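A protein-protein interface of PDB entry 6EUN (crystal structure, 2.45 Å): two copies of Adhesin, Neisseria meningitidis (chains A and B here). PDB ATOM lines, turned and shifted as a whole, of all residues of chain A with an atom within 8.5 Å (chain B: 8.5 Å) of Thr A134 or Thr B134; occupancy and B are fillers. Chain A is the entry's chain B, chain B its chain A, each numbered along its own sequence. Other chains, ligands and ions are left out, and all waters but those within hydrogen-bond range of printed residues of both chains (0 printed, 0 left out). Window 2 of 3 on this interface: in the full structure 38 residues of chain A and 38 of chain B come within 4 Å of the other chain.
Among the printed residues, merely in contact across the chains: Ile A127 with Ile B127, Phe A130 with Ala B131, Phe A130 with Thr B134, Phe A130 with Lys B135, Thr A134 with Thr B134 and Ile A141 with Ile B141.
Of chain B, only Thr B134 comes within 4 Å of Thr A134.
Of chain A, only Phe A130 and Thr A134 come within 4 Å of Thr B134.
Of the printed residues of chain A, Ile B127 touches Ile A127.
Of the printed residues of chain B, Phe A130 touches Ala B131, Thr B134 and Lys B135.
Of the printed residues of chain B, Ile A141 touches Ile B141 (3.7 Å).
OG1 of Thr B134 sits at hydrogen-bond distance from O of Phe B130 (2.7 Å).
The backbone carbonyl oxygen of Phe A130 lies within hydrogen-bond range of the side-chain hydroxyl of Thr A134.
Of the 16 printed residues of chain A, 4 touch a printed residue of chain B.
Hydrophobic or aromatic side chains of chain A within 4 Å of the printed part of chain B: Ile A127, Phe A130 and Ile A141.
Hydrophobic or aromatic side chains of chain B within 4 Å of the printed part of chain A: Ile B127, Ala B131 and Ile B141.
Among the printed residues, no Asp or Glu carboxylate lies within 4 Å of a Lys or Arg side-chain nitrogen of the other chain.
Ile A127 touches its own counterpart, Ile B127.
Phe A130 touches Thr B134, but with the chains exchanged Thr A134 does not touch Phe B130 (6.3 Å).
Phe A130 touches Lys B135, but with the chains exchanged Lys A135 does not touch Phe B130 (9.6 Å).
Thr B134 touches its own counterpart, Thr A134.
Of the 6 pairs that touch across the chains among the printed residues, 3 have their exchanged pair printed and touching as well.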
ATOM      1  N   ILE A 127      -5.271  -1.418  15.640  1.00  0.00           N
ATOM      2  CA  ILE A 127      -6.099  -0.335  16.228  1.00  0.00           C
ATOM      3  C   ILE A 127      -6.412  -0.634  17.656  1.00  0.00           C
ATOM      4  O   ILE A 127      -6.466   0.287  18.453  1.00  0.00           O
ATOM      5  CB  ILE A 127      -7.446  -0.092  15.475  1.00  0.00           C
ATOM      6  CG1 ILE A 127      -7.199   0.190  14.037  1.00  0.00           C
ATOM      7  CG2 ILE A 127      -8.121   1.111  16.082  1.00  0.00           C
ATOM      8  CD1 ILE A 127      -8.380  -0.233  13.181  1.00  0.00           C
ATOM      9  N   THR A 128      -6.761  -1.896  17.966  1.00  0.00           N
ATOM     10  CA  THR A 128      -7.053  -2.234  19.347  1.00  0.00           C
ATOM     11  C   THR A 128      -5.869  -1.889  20.278  1.00  0.00           C
ATOM     12  O   THR A 128      -6.086  -1.245  21.304  1.00  0.00           O
ATOM     13  CB  THR A 128      -7.501  -3.679  19.464  1.00  0.00           C
ATOM     14  OG1 THR A 128      -8.632  -3.878  18.609  1.00  0.00           O
ATOM     15  CG2 THR A 128      -7.813  -4.072  20.892  1.00  0.00           C
ATOM     16  N   THR A 129      -4.633  -2.235  19.871  1.00  0.00           N
ATOM     17  CA  THR A 129      -3.435  -1.977  20.669  1.00  0.00           C
ATOM     18  C   THR A 129      -3.235  -0.481  20.908  1.00  0.00           C
ATOM     19  O   THR A 129      -3.048  -0.051  22.067  1.00  0.00           O
ATOM     20  CB  THR A 129      -2.205  -2.611  20.021  1.00  0.00           C
ATOM     21  OG1 THR A 129      -2.461  -4.000  19.878  1.00  0.00           O
ATOM     22  CG2 THR A 129      -0.904  -2.373  20.848  1.00  0.00           C
ATOM     23  N   PHE A 130      -3.301   0.297  19.798  1.00  0.00           N
ATOM     24  CA  PHE A 130      -3.153   1.735  19.807  1.00  0.00           C
ATOM     25  C   PHE A 130      -4.186   2.407  20.732  1.00  0.00           C
ATOM     26  O   PHE A 130      -3.828   3.281  21.507  1.00  0.00           O
ATOM     27  CB  PHE A 130      -3.276   2.301  18.375  1.00  0.00           C
ATOM     28  CG  PHE A 130      -2.997   3.795  18.404  1.00  0.00           C
ATOM     29  CD1 PHE A 130      -1.689   4.278  18.559  1.00  0.00           C
ATOM     30  CD2 PHE A 130      -4.042   4.715  18.368  1.00  0.00           C
ATOM     31  CE1 PHE A 130      -1.444   5.659  18.663  1.00  0.00           C
ATOM     32  CE2 PHE A 130      -3.798   6.080  18.520  1.00  0.00           C
ATOM     33  CZ  PHE A 130      -2.502   6.543  18.667  1.00  0.00           C
ATOM     34  N   ALA A 131      -5.453   2.010  20.632  1.00  0.00           N
ATOM     35  CA  ALA A 131      -6.546   2.506  21.483  1.00  0.00           C
ATOM     36  C   ALA A 131      -6.246   2.194  22.951  1.00  0.00           C
ATOM     37  O   ALA A 131      -6.315   3.089  23.785  1.00  0.00           O
ATOM     38  CB  ALA A 131      -7.878   1.891  21.059  1.00  0.00           C
ATOM     39  N   GLU A 132      -5.782   0.980  23.250  1.00  0.00           N
ATOM     40  CA  GLU A 132      -5.416   0.604  24.628  1.00  0.00           C
ATOM     41  C   GLU A 132      -4.260   1.472  25.155  1.00  0.00           C
ATOM     42  O   GLU A 132      -4.354   1.975  26.266  1.00  0.00           O
ATOM     43  CB  GLU A 132      -5.050  -0.878  24.696  1.00  0.00           C
ATOM     44  CG  GLU A 132      -6.255  -1.795  24.581  1.00  0.00           C
ATOM     45  CD  GLU A 132      -5.935  -3.276  24.424  1.00  0.00           C
ATOM     46  OE1 GLU A 132      -6.596  -4.107  25.092  1.00  0.00           O
ATOM     47  OE2 GLU A 132      -5.057  -3.613  23.598  1.00  0.00           O
ATOM     48  N   GLU A 133      -3.205   1.714  24.340  1.00  0.00           N
ATOM     49  CA  GLU A 133      -2.068   2.529  24.757  1.00  0.00           C
ATOM     50  C   GLU A 133      -2.443   3.983  24.877  1.00  0.00           C
ATOM     51  O   GLU A 133      -1.940   4.660  25.767  1.00  0.00           O
ATOM     52  CB  GLU A 133      -0.902   2.362  23.804  1.00  0.00           C
ATOM     53  CG  GLU A 133      -0.266   0.984  23.867  1.00  0.00           C
ATOM     54  CD  GLU A 133       0.631   0.668  22.686  1.00  0.00           C
ATOM     55  OE1 GLU A 133       1.425  -0.297  22.797  1.00  0.00           O
ATOM     56  OE2 GLU A 133       0.515   1.351  21.638  1.00  0.00           O
ATOM     57  N   THR A 134      -3.342   4.485  24.009  1.00  0.00           N
ATOM     58  CA  THR A 134      -3.840   5.868  24.122  1.00  0.00           C
ATOM     59  C   THR A 134      -4.636   6.011  25.423  1.00  0.00           C
ATOM     60  O   THR A 134      -4.422   6.980  26.135  1.00  0.00           O
ATOM     61  CB  THR A 134      -4.723   6.218  22.944  1.00  0.00           C
ATOM     62  OG1 THR A 134      -3.987   5.975  21.775  1.00  0.00           O
ATOM     63  CG2 THR A 134      -5.141   7.636  22.957  1.00  0.00           C
ATOM     64  N   LYS A 135      -5.558   5.058  25.726  1.00  0.00           N
ATOM     65  CA  LYS A 135      -6.349   5.117  26.934  1.00  0.00           C
ATOM     66  C   LYS A 135      -5.424   5.223  28.166  1.00  0.00           C
ATOM     67  O   LYS A 135      -5.588   6.127  28.970  1.00  0.00           O
ATOM     68  CB  LYS A 135      -7.295   3.913  26.971  1.00  0.00           C
ATOM     69  CG  LYS A 135      -7.966   3.685  28.315  1.00  0.00           C
ATOM     70  CD  LYS A 135      -8.951   2.533  28.256  1.00  0.00           C
ATOM     71  CE  LYS A 135      -9.621   2.282  29.598  1.00  0.00           C
ATOM     72  NZ  LYS A 135     -10.401   1.011  29.591  1.00  0.00           N
ATOM     73  N   THR A 136      -4.421   4.343  28.271  1.00  0.00           N
ATOM     74  CA  THR A 136      -3.413   4.308  29.340  1.00  0.00           C
ATOM     75  C   THR A 136      -2.654   5.642  29.498  1.00  0.00           C
ATOM     76  O   THR A 136      -2.458   6.092  30.619  1.00  0.00           O
ATOM     77  CB  THR A 136      -2.460   3.135  29.073  1.00  0.00           C
ATOM     78  OG1 THR A 136      -3.189   1.930  29.263  1.00  0.00           O
ATOM     79  CG2 THR A 136      -1.263   3.117  29.978  1.00  0.00           C
ATOM     80  N   ASN A 137      -2.212   6.258  28.382  1.00  0.00           N
ATOM     81  CA  ASN A 137      -1.532   7.541  28.408  1.00  0.00           C
ATOM     82  C   ASN A 137      -2.435   8.656  28.886  1.00  0.00           C
ATOM     83  O   ASN A 137      -1.977   9.467  29.657  1.00  0.00           O
ATOM     84  CB  ASN A 137      -0.968   7.893  27.044  1.00  0.00           C
ATOM     85  CG  ASN A 137       0.219   7.070  26.645  1.00  0.00           C
ATOM     86  OD1 ASN A 137       1.014   6.664  27.464  1.00  0.00           O
ATOM     87  ND2 ASN A 137       0.384   6.824  25.367  1.00  0.00           N
ATOM     88  N   ILE A 138      -3.689   8.731  28.423  1.00  0.00           N
ATOM     89  CA  ILE A 138      -4.622   9.770  28.842  1.00  0.00           C
ATOM     90  C   ILE A 138      -4.921   9.658  30.327  1.00  0.00           C
ATOM     91  O   ILE A 138      -4.945  10.666  31.027  1.00  0.00           O
ATOM     92  CB  ILE A 138      -5.885   9.794  27.947  1.00  0.00           C
ATOM     93  CG1 ILE A 138      -5.514  10.354  26.552  1.00  0.00           C
ATOM     94  CG2 ILE A 138      -7.024  10.622  28.592  1.00  0.00           C
ATOM     95  CD1 ILE A 138      -6.537  10.054  25.470  1.00  0.00           C
ATOM     96  N   VAL A 139      -5.046   8.423  30.816  1.00  0.00           N
ATOM     97  CA  VAL A 139      -5.312   8.140  32.219  1.00  0.00           C
ATOM     98  C   VAL A 139      -4.096   8.545  33.098  1.00  0.00           C
ATOM     99  O   VAL A 139      -4.297   9.126  34.159  1.00  0.00           O
ATOM    100  CB  VAL A 139      -5.796   6.679  32.408  1.00  0.00           C
ATOM    101  CG1 VAL A 139      -5.631   6.207  33.852  1.00  0.00           C
ATOM    102  CG2 VAL A 139      -7.246   6.518  31.930  1.00  0.00           C
ATOM    103  N   LYS A 140      -2.869   8.275  32.647  1.00  0.00           N
ATOM    104  CA  LYS A 140      -1.676   8.684  33.381  1.00  0.00           C
ATOM    105  C   LYS A 140      -1.636  10.225  33.484  1.00  0.00           C
ATOM    106  O   LYS A 140      -1.459  10.741  34.588  1.00  0.00           O
ATOM    107  CB  LYS A 140      -0.396   8.175  32.710  1.00  0.00           C
ATOM    108  CG  LYS A 140      -0.097   6.721  32.990  1.00  0.00           C
ATOM    109  CD  LYS A 140       1.234   6.322  32.339  1.00  0.00           C
ATOM    110  CE  LYS A 140       1.523   4.837  32.376  1.00  0.00           C
ATOM    111  NZ  LYS A 140       2.816   4.519  31.711  1.00  0.00           N
ATOM    112  N   ILE A 141      -1.864  10.948  32.359  1.00  0.00           N
ATOM    113  CA  ILE A 141      -1.887  12.411  32.319  1.00  0.00           C
ATOM    114  C   ILE A 141      -2.936  12.976  33.309  1.00  0.00           C
ATOM    115  O   ILE A 141      -2.614  13.889  34.067  1.00  0.00           O
ATOM    116  CB  ILE A 141      -2.082  12.962  30.879  1.00  0.00           C
ATOM    117  CG1 ILE A 141      -0.874  12.692  29.995  1.00  0.00           C
ATOM    118  CG2 ILE A 141      -2.471  14.474  30.868  1.00  0.00           C
ATOM    119  CD1 ILE A 141      -1.231  12.739  28.545  1.00  0.00           C
ATOM    120  N   ASP A 142      -4.161  12.424  33.305  1.00  0.00           N
ATOM    121  CA  ASP A 142      -5.244  12.862  34.193  1.00  0.00           C
ATOM    122  C   ASP A 142      -4.850  12.726  35.660  1.00  0.00           C
ATOM    123  O   ASP A 142      -5.173  13.601  36.458  1.00  0.00           O
ATOM    124  CB  ASP A 142      -6.552  12.091  33.909  1.00  0.00           C
ATOM    125  CG  ASP A 142      -7.192  12.402  32.570  1.00  0.00           C
ATOM    126  OD1 ASP A 142      -6.822  13.427  31.954  1.00  0.00           O
ATOM    127  OD2 ASP A 142      -8.073  11.623  32.137  1.00  0.00           O
ATOM    128  N   ASN B 126      -6.464   6.662   7.026  1.00  0.00           N
ATOM    129  CA  ASN B 126      -7.059   7.598   7.980  1.00  0.00           C
ATOM    130  C   ASN B 126      -6.678   7.316   9.426  1.00  0.00           C
ATOM    131  O   ASN B 126      -6.422   8.259  10.173  1.00  0.00           O
ATOM    132  CB  ASN B 126      -8.567   7.595   7.806  1.00  0.00           C
ATOM    133  CG  ASN B 126      -9.004   8.274   6.544  1.00  0.00           C
ATOM    134  OD1 ASN B 126      -8.266   9.019   5.918  1.00  0.00           O
ATOM    135  ND2 ASN B 126     -10.219   8.051   6.151  1.00  0.00           N
ATOM    136  N   ILE B 127      -6.639   6.021   9.828  1.00  0.00           N
ATOM    137  CA  ILE B 127      -6.206   5.611  11.170  1.00  0.00           C
ATOM    138  C   ILE B 127      -4.755   5.947  11.343  1.00  0.00           C
ATOM    139  O   ILE B 127      -4.389   6.412  12.397  1.00  0.00           O
ATOM    140  CB  ILE B 127      -6.462   4.106  11.508  1.00  0.00           C
ATOM    141  CG1 ILE B 127      -7.888   3.764  11.327  1.00  0.00           C
ATOM    142  CG2 ILE B 127      -6.102   3.849  12.946  1.00  0.00           C
ATOM    143  CD1 ILE B 127      -8.104   2.395  10.934  1.00  0.00           C
ATOM    144  N   THR B 128      -3.903   5.692  10.339  1.00  0.00           N
ATOM    145  CA  THR B 128      -2.489   6.039  10.483  1.00  0.00           C
ATOM    146  C   THR B 128      -2.294   7.529  10.787  1.00  0.00           C
ATOM    147  O   THR B 128      -1.571   7.866  11.707  1.00  0.00           O
ATOM    148  CB  THR B 128      -1.667   5.563   9.290  1.00  0.00           C
ATOM    149  OG1 THR B 128      -1.947   4.184   9.106  1.00  0.00           O
ATOM    150  CG2 THR B 128      -0.163   5.807   9.484  1.00  0.00           C
ATOM    151  N   THR B 129      -2.974   8.404  10.061  1.00  0.00           N
ATOM    152  CA  THR B 129      -2.868   9.856  10.282  1.00  0.00           C
ATOM    153  C   THR B 129      -3.342  10.241  11.702  1.00  0.00           C
ATOM    154  O   THR B 129      -2.642  10.982  12.408  1.00  0.00           O
ATOM    155  CB  THR B 129      -3.679  10.580   9.209  1.00  0.00           C
ATOM    156  OG1 THR B 129      -3.234  10.102   7.926  1.00  0.00           O
ATOM    157  CG2 THR B 129      -3.607  12.156   9.352  1.00  0.00           C
ATOM    158  N   PHE B 130      -4.526   9.720  12.113  1.00  0.00           N
ATOM    159  CA  PHE B 130      -5.068   9.982  13.432  1.00  0.00           C
ATOM    160  C   PHE B 130      -4.114   9.513  14.526  1.00  0.00           C
ATOM    161  O   PHE B 130      -3.876  10.244  15.486  1.00  0.00           O
ATOM    162  CB  PHE B 130      -6.426   9.292  13.600  1.00  0.00           C
ATOM    163  CG  PHE B 130      -7.023   9.659  14.947  1.00  0.00           C
ATOM    164  CD1 PHE B 130      -7.594  10.919  15.156  1.00  0.00           C
ATOM    165  CD2 PHE B 130      -6.986   8.766  16.011  1.00  0.00           C
ATOM    166  CE1 PHE B 130      -8.088  11.276  16.421  1.00  0.00           C
ATOM    167  CE2 PHE B 130      -7.418   9.146  17.277  1.00  0.00           C
ATOM    168  CZ  PHE B 130      -7.974  10.391  17.472  1.00  0.00           C
ATOM    169  N   ALA B 131      -3.575   8.293  14.382  1.00  0.00           N
ATOM    170  CA  ALA B 131      -2.622   7.718  15.323  1.00  0.00           C
ATOM    171  C   ALA B 131      -1.357   8.609  15.412  1.00  0.00           C
ATOM    172  O   ALA B 131      -0.919   8.935  16.516  1.00  0.00           O
ATOM    173  CB  ALA B 131      -2.285   6.288  14.916  1.00  0.00           C
ATOM    174  N   GLU B 132      -0.830   9.073  14.260  1.00  0.00           N
ATOM    175  CA  GLU B 132       0.346   9.958  14.234  1.00  0.00           C
ATOM    176  C   GLU B 132       0.046  11.312  14.923  1.00  0.00           C
ATOM    177  O   GLU B 132       0.835  11.749  15.760  1.00  0.00           O
ATOM    178  CB  GLU B 132       0.814  10.199  12.809  1.00  0.00           C
ATOM    179  CG  GLU B 132       1.514   9.019  12.162  1.00  0.00           C
ATOM    180  CD  GLU B 132       1.820   9.255  10.688  1.00  0.00           C
ATOM    181  OE1 GLU B 132       3.013   9.314  10.315  1.00  0.00           O
ATOM    182  OE2 GLU B 132       0.858   9.462   9.918  1.00  0.00           O
ATOM    183  N   GLU B 133      -1.126  11.923  14.643  1.00  0.00           N
ATOM    184  CA  GLU B 133      -1.498  13.192  15.265  1.00  0.00           C
ATOM    185  C   GLU B 133      -1.758  13.030  16.738  1.00  0.00           C
ATOM    186  O   GLU B 133      -1.377  13.915  17.483  1.00  0.00           O
ATOM    187  CB  GLU B 133      -2.704  13.800  14.584  1.00  0.00           C
ATOM    188  CG  GLU B 133      -2.437  14.297  13.174  1.00  0.00           C
ATOM    189  CD  GLU B 133      -3.692  14.563  12.361  1.00  0.00           C
ATOM    190  OE1 GLU B 133      -3.591  15.286  11.338  1.00  0.00           O
ATOM    191  OE2 GLU B 133      -4.774  14.052  12.747  1.00  0.00           O
ATOM    192  N   THR B 134      -2.323  11.886  17.185  1.00  0.00           N
ATOM    193  CA  THR B 134      -2.513  11.581  18.624  1.00  0.00           C
ATOM    194  C   THR B 134      -1.159  11.434  19.356  1.00  0.00           C
ATOM    195  O   THR B 134      -1.035  11.975  20.458  1.00  0.00           O
ATOM    196  CB  THR B 134      -3.326  10.319  18.795  1.00  0.00           C
ATOM    197  OG1 THR B 134      -4.544  10.525  18.118  1.00  0.00           O
ATOM    198  CG2 THR B 134      -3.568   9.971  20.212  1.00  0.00           C
ATOM    199  N   LYS B 135      -0.168  10.702  18.783  1.00  0.00           N
ATOM    200  CA  LYS B 135       1.133  10.594  19.454  1.00  0.00           C
ATOM    201  C   LYS B 135       1.742  11.993  19.612  1.00  0.00           C
ATOM    202  O   LYS B 135       2.193  12.344  20.690  1.00  0.00           O
ATOM    203  CB  LYS B 135       2.136   9.681  18.693  1.00  0.00           C
ATOM    204  CG  LYS B 135       1.587   8.319  18.324  1.00  0.00           C
ATOM    205  CD  LYS B 135       2.585   7.576  17.448  1.00  0.00           C
ATOM    206  CE  LYS B 135       2.083   6.227  17.010  1.00  0.00           C
ATOM    207  NZ  LYS B 135       3.152   5.461  16.321  1.00  0.00           N
ATOM    208  N   THR B 136       1.746  12.796  18.544  1.00  0.00           N
ATOM    209  CA  THR B 136       2.276  14.154  18.597  1.00  0.00           C
ATOM    210  C   THR B 136       1.662  14.961  19.778  1.00  0.00           C
ATOM    211  O   THR B 136       2.409  15.607  20.522  1.00  0.00           O
ATOM    212  CB  THR B 136       2.030  14.826  17.255  1.00  0.00           C
ATOM    213  OG1 THR B 136       2.737  14.085  16.259  1.00  0.00           O
ATOM    214  CG2 THR B 136       2.476  16.247  17.238  1.00  0.00           C
ATOM    215  N   ASN B 137       0.312  14.899  19.944  1.00  0.00           N
ATOM    216  CA  ASN B 137      -0.404  15.610  20.989  1.00  0.00           C
ATOM    217  C   ASN B 137      -0.080  15.117  22.377  1.00  0.00           C
ATOM    218  O   ASN B 137       0.040  15.940  23.271  1.00  0.00           O
ATOM    219  CB  ASN B 137      -1.903  15.542  20.768  1.00  0.00           C
ATOM    220  CG  ASN B 137      -2.405  16.376  19.629  1.00  0.00           C
ATOM    221  OD1 ASN B 137      -1.816  17.364  19.235  1.00  0.00           O
ATOM    222  ND2 ASN B 137      -3.517  15.978  19.068  1.00  0.00           N
ATOM    223  N   ILE B 138      -0.003  13.793  22.589  1.00  0.00           N
ATOM    224  CA  ILE B 138       0.315  13.217  23.894  1.00  0.00           C
ATOM    225  C   ILE B 138       1.747  13.589  24.285  1.00  0.00           C
ATOM    226  O   ILE B 138       1.994  13.975  25.425  1.00  0.00           O
ATOM    227  CB  ILE B 138       0.019  11.697  23.940  1.00  0.00           C
ATOM    228  CG1 ILE B 138      -1.501  11.469  23.952  1.00  0.00           C
ATOM    229  CG2 ILE B 138       0.666  11.037  25.166  1.00  0.00           C
ATOM    230  CD1 ILE B 138      -1.962  10.093  23.545  1.00  0.00           C
ATOM    231  N   VAL B 139       2.658  13.562  23.300  1.00  0.00           N
ATOM    232  CA  VAL B 139       4.079  13.902  23.443  1.00  0.00           C
ATOM    233  C   VAL B 139       4.233  15.384  23.838  1.00  0.00           C
ATOM    234  O   VAL B 139       4.963  15.661  24.790  1.00  0.00           O
ATOM    235  CB  VAL B 139       4.892  13.470  22.193  1.00  0.00           C
ATOM    236  CG1 VAL B 139       6.166  14.303  22.003  1.00  0.00           C
ATOM    237  CG2 VAL B 139       5.197  11.967  22.238  1.00  0.00           C
ATOM    238  N   LYS B 140       3.478  16.299  23.181  1.00  0.00           N
ATOM    239  CA  LYS B 140       3.466  17.731  23.520  1.00  0.00           C
ATOM    240  C   LYS B 140       2.993  17.940  24.968  1.00  0.00           C
ATOM    241  O   LYS B 140       3.700  18.606  25.721  1.00  0.00           O
ATOM    242  CB  LYS B 140       2.581  18.534  22.571  1.00  0.00           C
ATOM    243  CG  LYS B 140       3.251  18.806  21.237  1.00  0.00           C
ATOM    244  CD  LYS B 140       2.373  19.704  20.360  1.00  0.00           C
ATOM    245  CE  LYS B 140       2.850  19.807  18.931  1.00  0.00           C
ATOM    246  NZ  LYS B 140       1.928  20.630  18.107  1.00  0.00           N
ATOM    247  N   ILE B 141       1.845  17.324  25.375  1.00  0.00           N
ATOM    248  CA  ILE B 141       1.321  17.401  26.745  1.00  0.00           C
ATOM    249  C   ILE B 141       2.381  16.889  27.755  1.00  0.00           C
ATOM    250  O   ILE B 141       2.602  17.537  28.773  1.00  0.00           O
ATOM    251  CB  ILE B 141      -0.021  16.632  26.901  1.00  0.00           C
ATOM    252  CG1 ILE B 141      -1.177  17.326  26.148  1.00  0.00           C
ATOM    253  CG2 ILE B 141      -0.359  16.376  28.376  1.00  0.00           C
ATOM    254  CD1 ILE B 141      -2.305  16.412  25.770  1.00  0.00           C
